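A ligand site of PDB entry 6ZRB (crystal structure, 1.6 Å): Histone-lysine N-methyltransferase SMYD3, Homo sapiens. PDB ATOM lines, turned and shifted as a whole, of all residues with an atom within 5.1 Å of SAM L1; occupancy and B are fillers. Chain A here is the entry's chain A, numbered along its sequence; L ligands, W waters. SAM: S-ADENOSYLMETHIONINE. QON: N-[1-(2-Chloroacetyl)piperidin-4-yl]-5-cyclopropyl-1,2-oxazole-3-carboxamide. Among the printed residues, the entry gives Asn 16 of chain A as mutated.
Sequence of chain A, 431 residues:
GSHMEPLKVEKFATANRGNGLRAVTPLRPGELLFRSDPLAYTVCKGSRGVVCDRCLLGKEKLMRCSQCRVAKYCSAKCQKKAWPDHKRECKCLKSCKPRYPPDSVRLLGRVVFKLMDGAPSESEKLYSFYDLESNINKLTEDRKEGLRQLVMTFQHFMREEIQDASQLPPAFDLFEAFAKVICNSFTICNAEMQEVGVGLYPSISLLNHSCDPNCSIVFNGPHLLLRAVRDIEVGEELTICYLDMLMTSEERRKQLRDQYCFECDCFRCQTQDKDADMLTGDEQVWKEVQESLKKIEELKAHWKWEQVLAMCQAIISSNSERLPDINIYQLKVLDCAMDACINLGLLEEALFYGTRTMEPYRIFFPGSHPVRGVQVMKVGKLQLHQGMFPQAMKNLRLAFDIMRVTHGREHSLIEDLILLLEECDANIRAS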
ATOM      1  N   ASN A  16      16.907 -28.639 -10.661  1.00  0.00           N
ATOM      2  CA  ASN A  16      15.533 -28.369 -10.182  1.00  0.00           C
ATOM      3  C   ASN A  16      14.729 -27.480 -11.115  1.00  0.00           C
ATOM      4  O   ASN A  16      13.710 -26.941 -10.673  1.00  0.00           O
ATOM      5  CB  ASN A  16      15.546 -27.788  -8.766  1.00  0.00           C
ATOM      6  CG  ASN A  16      16.334 -26.500  -8.643  1.00  0.00           C
ATOM      7  OD1 ASN A  16      16.247 -25.609  -9.492  1.00  0.00           O
ATOM      8  ND2 ASN A  16      17.097 -26.391  -7.581  1.00  0.00           N
ATOM      9  N   ARG A  17      15.114 -27.350 -12.375  1.00  0.00           N
ATOM     10  CA  ARG A  17      14.276 -26.567 -13.317  1.00  0.00           C
ATOM     11  C   ARG A  17      14.140 -27.332 -14.635  1.00  0.00           C
ATOM     12  O   ARG A  17      14.005 -26.695 -15.691  1.00  0.00           O
ATOM     13  CB  ARG A  17      14.785 -25.138 -13.489  1.00  0.00           C
ATOM     14  CG  ARG A  17      16.275 -24.926 -13.355  1.00  0.00           C
ATOM     15  CD  ARG A  17      16.644 -23.478 -13.597  1.00  0.00           C
ATOM     16  NE  ARG A  17      16.878 -22.683 -12.403  1.00  0.00           N
ATOM     17  CZ  ARG A  17      17.749 -21.672 -12.324  1.00  0.00           C
ATOM     18  NH1 ARG A  17      17.879 -20.996 -11.199  1.00  0.00           N
ATOM     19  NH2 ARG A  17      18.518 -21.361 -13.365  1.00  0.00           N
ATOM     20  N   GLY A  18      14.090 -28.655 -14.563  1.00  0.00           N
ATOM     21  CA  GLY A  18      13.904 -29.510 -15.727  1.00  0.00           C
ATOM     22  C   GLY A  18      15.079 -29.421 -16.655  1.00  0.00           C
ATOM     23  O   GLY A  18      16.224 -29.392 -16.180  1.00  0.00           O
ATOM     24  N   ASN A  19      14.837 -29.463 -17.951  1.00  0.00           N
ATOM     25  CA  ASN A  19      15.930 -29.381 -18.942  1.00  0.00           C
ATOM     26  C   ASN A  19      16.317 -27.924 -19.110  1.00  0.00           C
ATOM     27  O   ASN A  19      15.488 -27.023 -18.834  1.00  0.00           O
ATOM     28  CB  ASN A  19      15.534 -30.009 -20.280  1.00  0.00           C
ATOM     29  CG  ASN A  19      15.279 -31.484 -20.136  1.00  0.00           C
ATOM     30  OD1 ASN A  19      16.044 -32.186 -19.466  1.00  0.00           O
ATOM     31  ND2 ASN A  19      14.196 -31.968 -20.709  1.00  0.00           N
ATOM     32  N   GLY A  20      17.557 -27.698 -19.514  1.00  0.00           N
ATOM     33  CA  GLY A  20      18.060 -26.351 -19.805  1.00  0.00           C
ATOM     34  C   GLY A  20      19.098 -26.370 -20.902  1.00  0.00           C
ATOM     35  O   GLY A  20      19.366 -27.455 -21.451  1.00  0.00           O
ATOM     36  N   TYR A 127      15.590 -29.847 -29.378  1.00  0.00           N
ATOM     37  CA  TYR A 127      14.396 -30.105 -28.532  1.00  0.00           C
ATOM     38  C   TYR A 127      13.178 -29.979 -29.420  1.00  0.00           C
ATOM     39  O   TYR A 127      13.142 -29.040 -30.233  1.00  0.00           O
ATOM     40  CB  TYR A 127      14.332 -29.066 -27.408  1.00  0.00           C
ATOM     41  CG  TYR A 127      13.724 -29.451 -26.086  1.00  0.00           C
ATOM     42  CD1 TYR A 127      14.094 -30.606 -25.407  1.00  0.00           C
ATOM     43  CD2 TYR A 127      12.858 -28.584 -25.417  1.00  0.00           C
ATOM     44  CE1 TYR A 127      13.621 -30.903 -24.139  1.00  0.00           C
ATOM     45  CE2 TYR A 127      12.377 -28.868 -24.156  1.00  0.00           C
ATOM     46  CZ  TYR A 127      12.755 -30.040 -23.508  1.00  0.00           C
ATOM     47  OH  TYR A 127      12.341 -30.270 -22.236  1.00  0.00           O
ATOM     48  N   ASP A 131       8.903 -32.882 -26.864  1.00  0.00           N
ATOM     49  CA  ASP A 131       9.737 -32.814 -25.641  1.00  0.00           C
ATOM     50  C   ASP A 131       9.281 -31.679 -24.713  1.00  0.00           C
ATOM     51  O   ASP A 131       9.728 -31.688 -23.546  1.00  0.00           O
ATOM     52  CB  ASP A 131      11.201 -32.554 -26.002  1.00  0.00           C
ATOM     53  CG  ASP A 131      11.885 -33.639 -26.816  1.00  0.00           C
ATOM     54  OD1 ASP A 131      11.554 -34.840 -26.596  1.00  0.00           O
ATOM     55  OD2 ASP A 131      12.748 -33.268 -27.653  1.00  0.00           O
ATOM     56  N   LEU A 132       8.526 -30.711 -25.221  1.00  0.00           N
ATOM     57  CA  LEU A 132       8.290 -29.453 -24.475  1.00  0.00           C
ATOM     58  C   LEU A 132       7.630 -29.742 -23.129  1.00  0.00           C
ATOM     59  O   LEU A 132       6.749 -30.637 -23.028  1.00  0.00           O
ATOM     60  CB  LEU A 132       7.403 -28.506 -25.284  1.00  0.00           C
ATOM     61  CG  LEU A 132       8.037 -27.928 -26.543  1.00  0.00           C
ATOM     62  CD1 LEU A 132       7.033 -27.040 -27.263  1.00  0.00           C
ATOM     63  CD2 LEU A 132       9.316 -27.162 -26.202  1.00  0.00           C
ATOM     64  N   GLU A 133       8.010 -28.942 -22.146  1.00  0.00           N
ATOM     65  CA  GLU A 133       7.386 -28.941 -20.810  1.00  0.00           C
ATOM     66  C   GLU A 133       5.923 -28.517 -20.907  1.00  0.00           C
ATOM     67  O   GLU A 133       5.597 -27.503 -21.552  1.00  0.00           O
ATOM     68  CB  GLU A 133       8.149 -27.995 -19.895  1.00  0.00           C
ATOM     69  CG  GLU A 133       7.548 -27.887 -18.504  1.00  0.00           C
ATOM     70  CD  GLU A 133       7.681 -29.175 -17.717  1.00  0.00           C
ATOM     71  OE1 GLU A 133       8.838 -29.489 -17.329  1.00  0.00           O
ATOM     72  OE2 GLU A 133       6.651 -29.888 -17.534  1.00  0.00           O
ATOM     73  N   ASN A 135       4.004 -28.791 -17.707  1.00  0.00           N
ATOM     74  CA  ASN A 135       3.628 -28.495 -16.303  1.00  0.00           C
ATOM     75  C   ASN A 135       2.259 -29.056 -15.943  1.00  0.00           C
ATOM     76  O   ASN A 135       1.595 -28.466 -15.056  1.00  0.00           O
ATOM     77  CB  ASN A 135       3.658 -26.987 -16.040  1.00  0.00           C
ATOM     78  CG  ASN A 135       5.073 -26.464 -16.032  1.00  0.00           C
ATOM     79  OD1 ASN A 135       5.906 -27.020 -15.330  1.00  0.00           O
ATOM     80  ND2 ASN A 135       5.313 -25.422 -16.806  1.00  0.00           N
ATOM     81  N   CYS A 183       3.294 -22.319 -21.907  1.00  0.00           N
ATOM     82  CA  CYS A 183       4.581 -22.041 -21.232  1.00  0.00           C
ATOM     83  C   CYS A 183       5.749 -22.114 -22.213  1.00  0.00           C
ATOM     84  O   CYS A 183       6.887 -22.014 -21.746  1.00  0.00           O
ATOM     85  CB  CYS A 183       4.791 -22.914 -20.013  1.00  0.00           C
ATOM     86  SG  CYS A 183       4.891 -24.674 -20.405  1.00  0.00           S
ATOM     87  N   ASN A 184       5.504 -22.170 -23.518  1.00  0.00           N
ATOM     88  CA  ASN A 184       6.596 -22.217 -24.530  1.00  0.00           C
ATOM     89  C   ASN A 184       6.366 -21.258 -25.710  1.00  0.00           C
ATOM     90  O   ASN A 184       7.242 -21.223 -26.561  1.00  0.00           O
ATOM     91  CB  ASN A 184       6.801 -23.633 -25.060  1.00  0.00           C
ATOM     92  CG  ASN A 184       7.366 -24.543 -23.983  1.00  0.00           C
ATOM     93  OD1 ASN A 184       8.554 -24.452 -23.680  1.00  0.00           O
ATOM     94  ND2 ASN A 184       6.539 -25.380 -23.386  1.00  0.00           N
ATOM     95  N   SER A 205      13.173 -23.062 -26.593  1.00  0.00           N
ATOM     96  CA  SER A 205      12.346 -23.391 -25.408  1.00  0.00           C
ATOM     97  C   SER A 205      13.155 -24.092 -24.333  1.00  0.00           C
ATOM     98  O   SER A 205      12.624 -24.188 -23.228  1.00  0.00           O
ATOM     99  CB  SER A 205      11.173 -24.262 -25.752  1.00  0.00           C
ATOM    100  OG  SER A 205      10.164 -23.490 -26.327  1.00  0.00           O
ATOM    101  N   LEU A 206      14.367 -24.572 -24.596  1.00  0.00           N
ATOM    102  CA  LEU A 206      15.233 -25.134 -23.518  1.00  0.00           C
ATOM    103  C   LEU A 206      15.646 -24.061 -22.531  1.00  0.00           C
ATOM    104  O   LEU A 206      16.009 -24.422 -21.391  1.00  0.00           O
ATOM    105  CB  LEU A 206      16.457 -25.829 -24.111  1.00  0.00           C
ATOM    106  CG  LEU A 206      16.191 -27.258 -24.561  1.00  0.00           C
ATOM    107  CD1 LEU A 206      17.363 -27.758 -25.383  1.00  0.00           C
ATOM    108  CD2 LEU A 206      15.912 -28.155 -23.374  1.00  0.00           C
ATOM    109  N   LEU A 207      15.673 -22.787 -22.923  1.00  0.00           N
ATOM    110  CA  LEU A 207      16.217 -21.734 -22.021  1.00  0.00           C
ATOM    111  C   LEU A 207      15.297 -21.540 -20.817  1.00  0.00           C
ATOM    112  O   LEU A 207      14.144 -21.184 -20.983  1.00  0.00           O
ATOM    113  CB  LEU A 207      16.351 -20.424 -22.772  1.00  0.00           C
ATOM    114  CG  LEU A 207      17.442 -20.408 -23.835  1.00  0.00           C
ATOM    115  CD1 LEU A 207      17.124 -19.363 -24.888  1.00  0.00           C
ATOM    116  CD2 LEU A 207      18.800 -20.165 -23.187  1.00  0.00           C
ATOM    117  N   ASN A 208      15.860 -21.669 -19.622  1.00  0.00           N
ATOM    118  CA  ASN A 208      15.174 -21.271 -18.387  1.00  0.00           C
ATOM    119  C   ASN A 208      15.266 -19.755 -18.172  1.00  0.00           C
ATOM    120  O   ASN A 208      16.033 -19.050 -18.845  1.00  0.00           O
ATOM    121  CB  ASN A 208      15.735 -22.083 -17.223  1.00  0.00           C
ATOM    122  CG  ASN A 208      15.263 -23.521 -17.316  1.00  0.00           C
ATOM    123  OD1 ASN A 208      14.080 -23.766 -17.581  1.00  0.00           O
ATOM    124  ND2 ASN A 208      16.166 -24.477 -17.145  1.00  0.00           N
ATOM    125  N   HIS A 209      14.440 -19.275 -17.260  1.00  0.00           N
ATOM    126  CA  HIS A 209      14.233 -17.843 -16.953  1.00  0.00           C
ATOM    127  C   HIS A 209      15.197 -17.346 -15.890  1.00  0.00           C
ATOM    128  O   HIS A 209      15.436 -18.052 -14.898  1.00  0.00           O
ATOM    129  CB  HIS A 209      12.808 -17.648 -16.459  1.00  0.00           C
ATOM    130  CG  HIS A 209      12.595 -16.306 -15.857  1.00  0.00           C
ATOM    131  ND1 HIS A 209      12.327 -15.181 -16.625  1.00  0.00           N
ATOM    132  CD2 HIS A 209      12.666 -15.904 -14.568  1.00  0.00           C
ATOM    133  CE1 HIS A 209      12.225 -14.137 -15.824  1.00  0.00           C
ATOM    134  NE2 HIS A 209      12.416 -14.565 -14.540  1.00  0.00           N
ATOM    135  N   SER A 210      15.609 -16.095 -16.034  1.00  0.00           N
ATOM    136  CA  SER A 210      16.193 -15.301 -14.929  1.00  0.00           C
ATOM    137  C   SER A 210      15.693 -13.869 -15.042  1.00  0.00           C
ATOM    138  O   SER A 210      15.578 -13.379 -16.171  1.00  0.00           O
ATOM    139  CB  SER A 210      17.672 -15.345 -14.992  1.00  0.00           C
ATOM    140  OG  SER A 210      18.215 -14.473 -14.009  1.00  0.00           O
ATOM    141  N   TYR A 242      11.993 -14.089 -19.373  1.00  0.00           N
ATOM    142  CA  TYR A 242      10.710 -14.356 -20.076  1.00  0.00           C
ATOM    143  C   TYR A 242       9.808 -13.117 -20.055  1.00  0.00           C
ATOM    144  O   TYR A 242       8.780 -13.083 -20.784  1.00  0.00           O
ATOM    145  CB  TYR A 242       9.960 -15.476 -19.342  1.00  0.00           C
ATOM    146  CG  TYR A 242      10.553 -16.865 -19.414  1.00  0.00           C
ATOM    147  CD1 TYR A 242      11.739 -17.157 -20.064  1.00  0.00           C
ATOM    148  CD2 TYR A 242       9.911 -17.907 -18.763  1.00  0.00           C
ATOM    149  CE1 TYR A 242      12.245 -18.451 -20.099  1.00  0.00           C
ATOM    150  CE2 TYR A 242      10.399 -19.197 -18.784  1.00  0.00           C
ATOM    151  CZ  TYR A 242      11.570 -19.474 -19.473  1.00  0.00           C
ATOM    152  OH  TYR A 242      12.041 -20.767 -19.494  1.00  0.00           O
ATOM    153  N   TYR A 260       3.869 -19.958 -15.999  1.00  0.00           N
ATOM    154  CA  TYR A 260       5.068 -20.836 -16.079  1.00  0.00           C
ATOM    155  C   TYR A 260       5.144 -21.819 -14.919  1.00  0.00           C
ATOM    156  O   TYR A 260       6.049 -22.648 -14.929  1.00  0.00           O
ATOM    157  CB  TYR A 260       6.341 -19.998 -16.211  1.00  0.00           C
ATOM    158  CG  TYR A 260       6.369 -19.220 -17.506  1.00  0.00           C
ATOM    159  CD1 TYR A 260       6.588 -19.886 -18.694  1.00  0.00           C
ATOM    160  CD2 TYR A 260       6.134 -17.849 -17.554  1.00  0.00           C
ATOM    161  CE1 TYR A 260       6.611 -19.198 -19.896  1.00  0.00           C
ATOM    162  CE2 TYR A 260       6.128 -17.159 -18.758  1.00  0.00           C
ATOM    163  CZ  TYR A 260       6.378 -17.835 -19.932  1.00  0.00           C
ATOM    164  OH  TYR A 260       6.363 -17.161 -21.129  1.00  0.00           O
ATOM    165  N   CYS A 261       4.225 -21.765 -13.963  1.00  0.00           N
ATOM    166  CA  CYS A 261       4.185 -22.696 -12.817  1.00  0.00           C
ATOM    167  C   CYS A 261       5.545 -22.824 -12.137  1.00  0.00           C
ATOM    168  O   CYS A 261       5.978 -23.956 -11.844  1.00  0.00           O
ATOM    169  CB  CYS A 261       3.713 -24.083 -13.251  1.00  0.00           C
ATOM    170  SG  CYS A 261       2.017 -24.070 -13.875  1.00  0.00           S
ATOM    171  N   PHE A 262       6.220 -21.702 -11.861  1.00  0.00           N
ATOM    172  CA  PHE A 262       7.381 -21.770 -10.932  1.00  0.00           C
ATOM    173  C   PHE A 262       7.461 -20.519 -10.073  1.00  0.00           C
ATOM    174  O   PHE A 262       6.855 -19.473 -10.383  1.00  0.00           O
ATOM    175  CB  PHE A 262       8.694 -22.091 -11.640  1.00  0.00           C
ATOM    176  CG  PHE A 262       9.280 -20.950 -12.439  1.00  0.00           C
ATOM    177  CD1 PHE A 262       8.900 -20.748 -13.749  1.00  0.00           C
ATOM    178  CD2 PHE A 262      10.208 -20.089 -11.871  1.00  0.00           C
ATOM    179  CE1 PHE A 262       9.436 -19.715 -14.495  1.00  0.00           C
ATOM    180  CE2 PHE A 262      10.745 -19.062 -12.630  1.00  0.00           C
ATOM    181  CZ  PHE A 262      10.348 -18.862 -13.941  1.00  0.00           C
ATOM    182  N   GLU A 263       8.211 -20.696  -8.993  1.00  0.00           N
ATOM    183  CA  GLU A 263       8.524 -19.675  -7.965  1.00  0.00           C
ATOM    184  C   GLU A 263       9.969 -19.227  -8.216  1.00  0.00           C
ATOM    185  O   GLU A 263      10.849 -20.081  -8.231  1.00  0.00           O
ATOM    186  CB  GLU A 263       8.379 -20.281  -6.573  1.00  0.00           C
ATOM    187  CG  GLU A 263       7.123 -21.140  -6.416  1.00  0.00           C
ATOM    188  CD  GLU A 263       5.834 -20.375  -6.516  1.00  0.00           C
ATOM    189  OE1 GLU A 263       5.871 -19.110  -6.540  1.00  0.00           O
ATOM    190  OE2 GLU A 263       4.791 -21.020  -6.588  1.00  0.00           O
ATOM    191  N   CYS A 264      10.197 -17.955  -8.535  1.00  0.00           N
ATOM    192  CA  CYS A 264      11.551 -17.514  -8.944  1.00  0.00           C
ATOM    193  C   CYS A 264      12.390 -17.274  -7.703  1.00  0.00           C
ATOM    194  O   CYS A 264      11.960 -16.489  -6.835  1.00  0.00           O
ATOM    195  CB  CYS A 264      11.536 -16.270  -9.805  1.00  0.00           C
ATOM    196  SG  CYS A 264      13.193 -15.920 -10.490  1.00  0.00           S
HETATM  197  N   SAM L   1      12.886 -26.318 -18.103  1.00  0.00           N
HETATM  198  CA  SAM L   1      12.109 -26.349 -19.371  1.00  0.00           C
HETATM  199  C   SAM L   1      12.082 -27.781 -19.938  1.00  0.00           C
HETATM  200  O   SAM L   1      11.602 -27.946 -21.076  1.00  0.00           O
HETATM  201  OXT SAM L   1      12.441 -28.701 -19.170  1.00  0.00           O
HETATM  202  CB  SAM L   1      12.708 -25.371 -20.375  1.00  0.00           C
HETATM  203  CG  SAM L   1      12.186 -23.938 -20.195  1.00  0.00           C
HETATM  204  SD  SAM L   1      10.422 -23.882 -20.656  1.00  0.00           S
HETATM  205  CE  SAM L   1      10.409 -22.531 -21.836  1.00  0.00           C
HETATM  206  C5' SAM L   1       9.667 -23.039 -19.244  1.00  0.00           C
HETATM  207  C4' SAM L   1       9.514 -23.883 -18.002  1.00  0.00           C
HETATM  208  O4' SAM L   1      10.810 -24.162 -17.445  1.00  0.00           O
HETATM  209  C3' SAM L   1       8.732 -23.225 -16.865  1.00  0.00           C
HETATM  210  O3' SAM L   1       7.337 -23.366 -17.111  1.00  0.00           O
HETATM  211  C2' SAM L   1       9.259 -24.038 -15.687  1.00  0.00           C
HETATM  212  O2' SAM L   1       8.738 -25.352 -15.659  1.00  0.00           O
HETATM  213  C1' SAM L   1      10.745 -24.093 -16.031  1.00  0.00           C
HETATM  214  N9  SAM L   1      11.530 -22.942 -15.577  1.00  0.00           N
HETATM  215  C8  SAM L   1      12.017 -21.935 -16.360  1.00  0.00           C
HETATM  216  N7  SAM L   1      12.772 -21.084 -15.713  1.00  0.00           N
HETATM  217  C5  SAM L   1      12.742 -21.554 -14.399  1.00  0.00           C
HETATM  218  C6  SAM L   1      13.323 -21.058 -13.208  1.00  0.00           C
HETATM  219  N6  SAM L   1      14.106 -19.988 -13.152  1.00  0.00           N
HETATM  220  N1  SAM L   1      13.111 -21.786 -12.076  1.00  0.00           N
HETATM  221  C2  SAM L   1      12.363 -22.892 -12.146  1.00  0.00           C
HETATM  222  N3  SAM L   1      11.751 -23.423 -13.199  1.00  0.00           N
HETATM  223  C4  SAM L   1      12.000 -22.705 -14.309  1.00  0.00           C
HETATM  224  C11 QON L   2       9.041 -13.980 -25.018  1.00  0.00           C
HETATM  225  C13 QON L   2       9.573 -15.142 -24.273  1.00  0.00           C
HETATM  226  C17 QON L   2       9.028 -16.442 -24.153  1.00  0.00           C
HETATM  227  C19 QON L   2       9.340 -19.623 -23.864  1.00  0.00           C
HETATM  228  C01 QON L   2       9.275  -7.175 -27.998  1.00  0.00           C
HETATM  229  C02 QON L   2      10.290  -8.254 -27.983  1.00  0.00           C
HETATM  230  O03 QON L   2      11.369  -8.030 -28.504  1.00  0.00           O
HETATM  231  N04 QON L   2       9.951  -9.470 -27.494  1.00  0.00           N
HETATM  232  C05 QON L   2      10.911 -10.549 -27.777  1.00  0.00           C
HETATM  233  C06 QON L   2      11.071 -11.476 -26.606  1.00  0.00           C
HETATM  234  C07 QON L   2       9.699 -11.950 -26.184  1.00  0.00           C
HETATM  235  C08 QON L   2       8.842 -10.800 -25.718  1.00  0.00           C
HETATM  236  C09 QON L   2       8.663  -9.760 -26.839  1.00  0.00           C
HETATM  237  N10 QON L   2       9.852 -12.917 -25.120  1.00  0.00           N
HETATM  238  O12 QON L   2       7.964 -14.069 -25.556  1.00  0.00           O
HETATM  239  N14 QON L   2      10.766 -15.100 -23.646  1.00  0.00           N
HETATM  240  O15 QON L   2      10.943 -16.310 -23.108  1.00  0.00           O
HETATM  241  C16 QON L   2       9.941 -17.152 -23.432  1.00  0.00           C
HETATM  242  C18 QON L   2       9.947 -18.560 -22.947  1.00  0.00           C
HETATM  243  C20 QON L   2       8.659 -19.214 -22.596  1.00  0.00           C
HETATM  244  O   HOH W   1      13.353 -24.373  -9.144  1.00  0.00           O
HETATM  245  O   HOH W   2      10.287 -25.666 -12.245  1.00  0.00           O
HETATM  246  O   HOH W   3      15.224 -18.505 -10.852  1.00  0.00           O
HETATM  247  O   HOH W   4      13.428 -20.876  -9.319  1.00  0.00           O
HETATM  248  O   HOH W   5       7.481 -25.660 -13.222  1.00  0.00           O
HETATM  249  O   HOH W   6      10.946 -30.900 -18.896  1.00  0.00           O
HETATM  250  O   HOH W   7       9.777 -26.833 -22.760  1.00  0.00           O
HETATM  251  O   HOH W   8      10.719 -27.466 -16.535  1.00  0.00           O
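O3' of SAM L1 is in hydrogen-bond range of O of Tyr 260 (2.6 Å). A nitrogen (N7) of SAM L1 sits at hydrogen-bond distance from the backbone NH (N) of His 209, 2.9 Å away. O of SAM L1 lies within hydrogen-bond range of OH of Tyr 127 (2.7 Å). The side-chain amide oxygen (OD1) of Asn 208 lies within hydrogen-bond range of a nitrogen (N) of SAM L1, 2.9 Å away. The backbone carbonyl oxygen of Asn 19 sits at hydrogen-bond distance from a nitrogen (N) of SAM L1 (2.8 Å). The side-chain amide nitrogen (ND2) of Asn 135 is in hydrogen-bond range of an oxygen (O3') of SAM L1. O of Arg 17 sits at hydrogen-bond distance from N of SAM L1, at 2.7 Å. N6 of SAM L1 sits at hydrogen-bond distance from O of His 209 (2.9 Å). An oxygen (OXT) of SAM L1 is in hydrogen-bond range of the backbone NH of Asn 19 (2.8 Å).
The side-chain sulfur (SG) of Cys 183 lies within hydrogen-bond range of the side-chain amide nitrogen (ND2) of Asn 135. OG of Ser 205 lies within hydrogen-bond range of OD1 of Asn 184 (3.2 Å). The backbone carbonyl oxygen (O) of Leu 207 is in hydrogen-bond range of the side-chain hydroxyl (OH) of Tyr 242 (2.6 Å). The backbone carbonyl oxygen of Glu 133 sits at hydrogen-bond distance from the side-chain sulfur of Cys 183 (3.1 Å). N of Asn 135 sits at hydrogen-bond distance from OE2 of Glu 133. O of Asn 19 sits at hydrogen-bond distance from ND2 of Asn 208, 3.1 Å away. O of Arg 17 lies within hydrogen-bond range of ND2 of Asn 208, at 3.4 Å. The backbone carbonyl oxygen (O) of Asp 131 is in hydrogen-bond range of the side-chain hydroxyl (OH) of Tyr 127, 3.2 Å away.
OD1 of Asn 184 sits close to SD of SAM L1 (3.6 Å). O of Ser 205 sits close to SD of SAM L1 (3.4 Å). The side-chain hydroxyl (OH) of Tyr 242 sits close to a sulfur (SD) of SAM L1 (3.7 Å). Gly 18 touches SAM L1. Glu 133 touches SAM L1 (CB to O, 3.6 Å). Cys 183 touches SAM L1 (O to CE, 3.6 Å). Leu 206 touches SAM L1 (O to CB, 3.6 Å). Leu 207 touches SAM L1. Phe 262 touches SAM L1. Hydrophobic or aromatic side chains within 4 Å of SAM L1: Tyr 127, His 209, Tyr 242, Tyr 260 and Phe 262. 16 residues have an atom within 4 Å of SAM L1: Arg 17, Gly 18, Asn 19, Tyr 127, Glu 133, Asn 135, Cys 183, Asn 184, Ser 205, Leu 206, Leu 207, Asn 208, His 209, Tyr 242, Tyr 260 and Phe 262. The nearest printed residue that does not touch SAM L1 is Asn 16 (4.5 Å).
Water W6 lies within hydrogen-bond range of an oxygen (OXT) of SAM L1 (2.7 Å) and the side-chain carboxylate of Glu 133 (3.0 Å). Water W7 lies within hydrogen-bond range of an oxygen (O) of SAM L1, the backbone NH (N) of Glu 133 and the side-chain amide oxygen (OD1) of Asn 184. Water W5 lies within hydrogen-bond range of O of Cys 261 (2.7 Å), O2' of SAM L1 (2.8 Å) and OD1 of Asn 135 (3.0 Å). Water W8 lies within hydrogen-bond range of the side-chain carboxylate of Glu 133, a nitrogen (N) of SAM L1 and the backbone carbonyl oxygen of Arg 17. Water W4 lies within hydrogen-bond range of O of Glu 263 (2.9 Å) and N1 of SAM L1 (2.9 Å).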
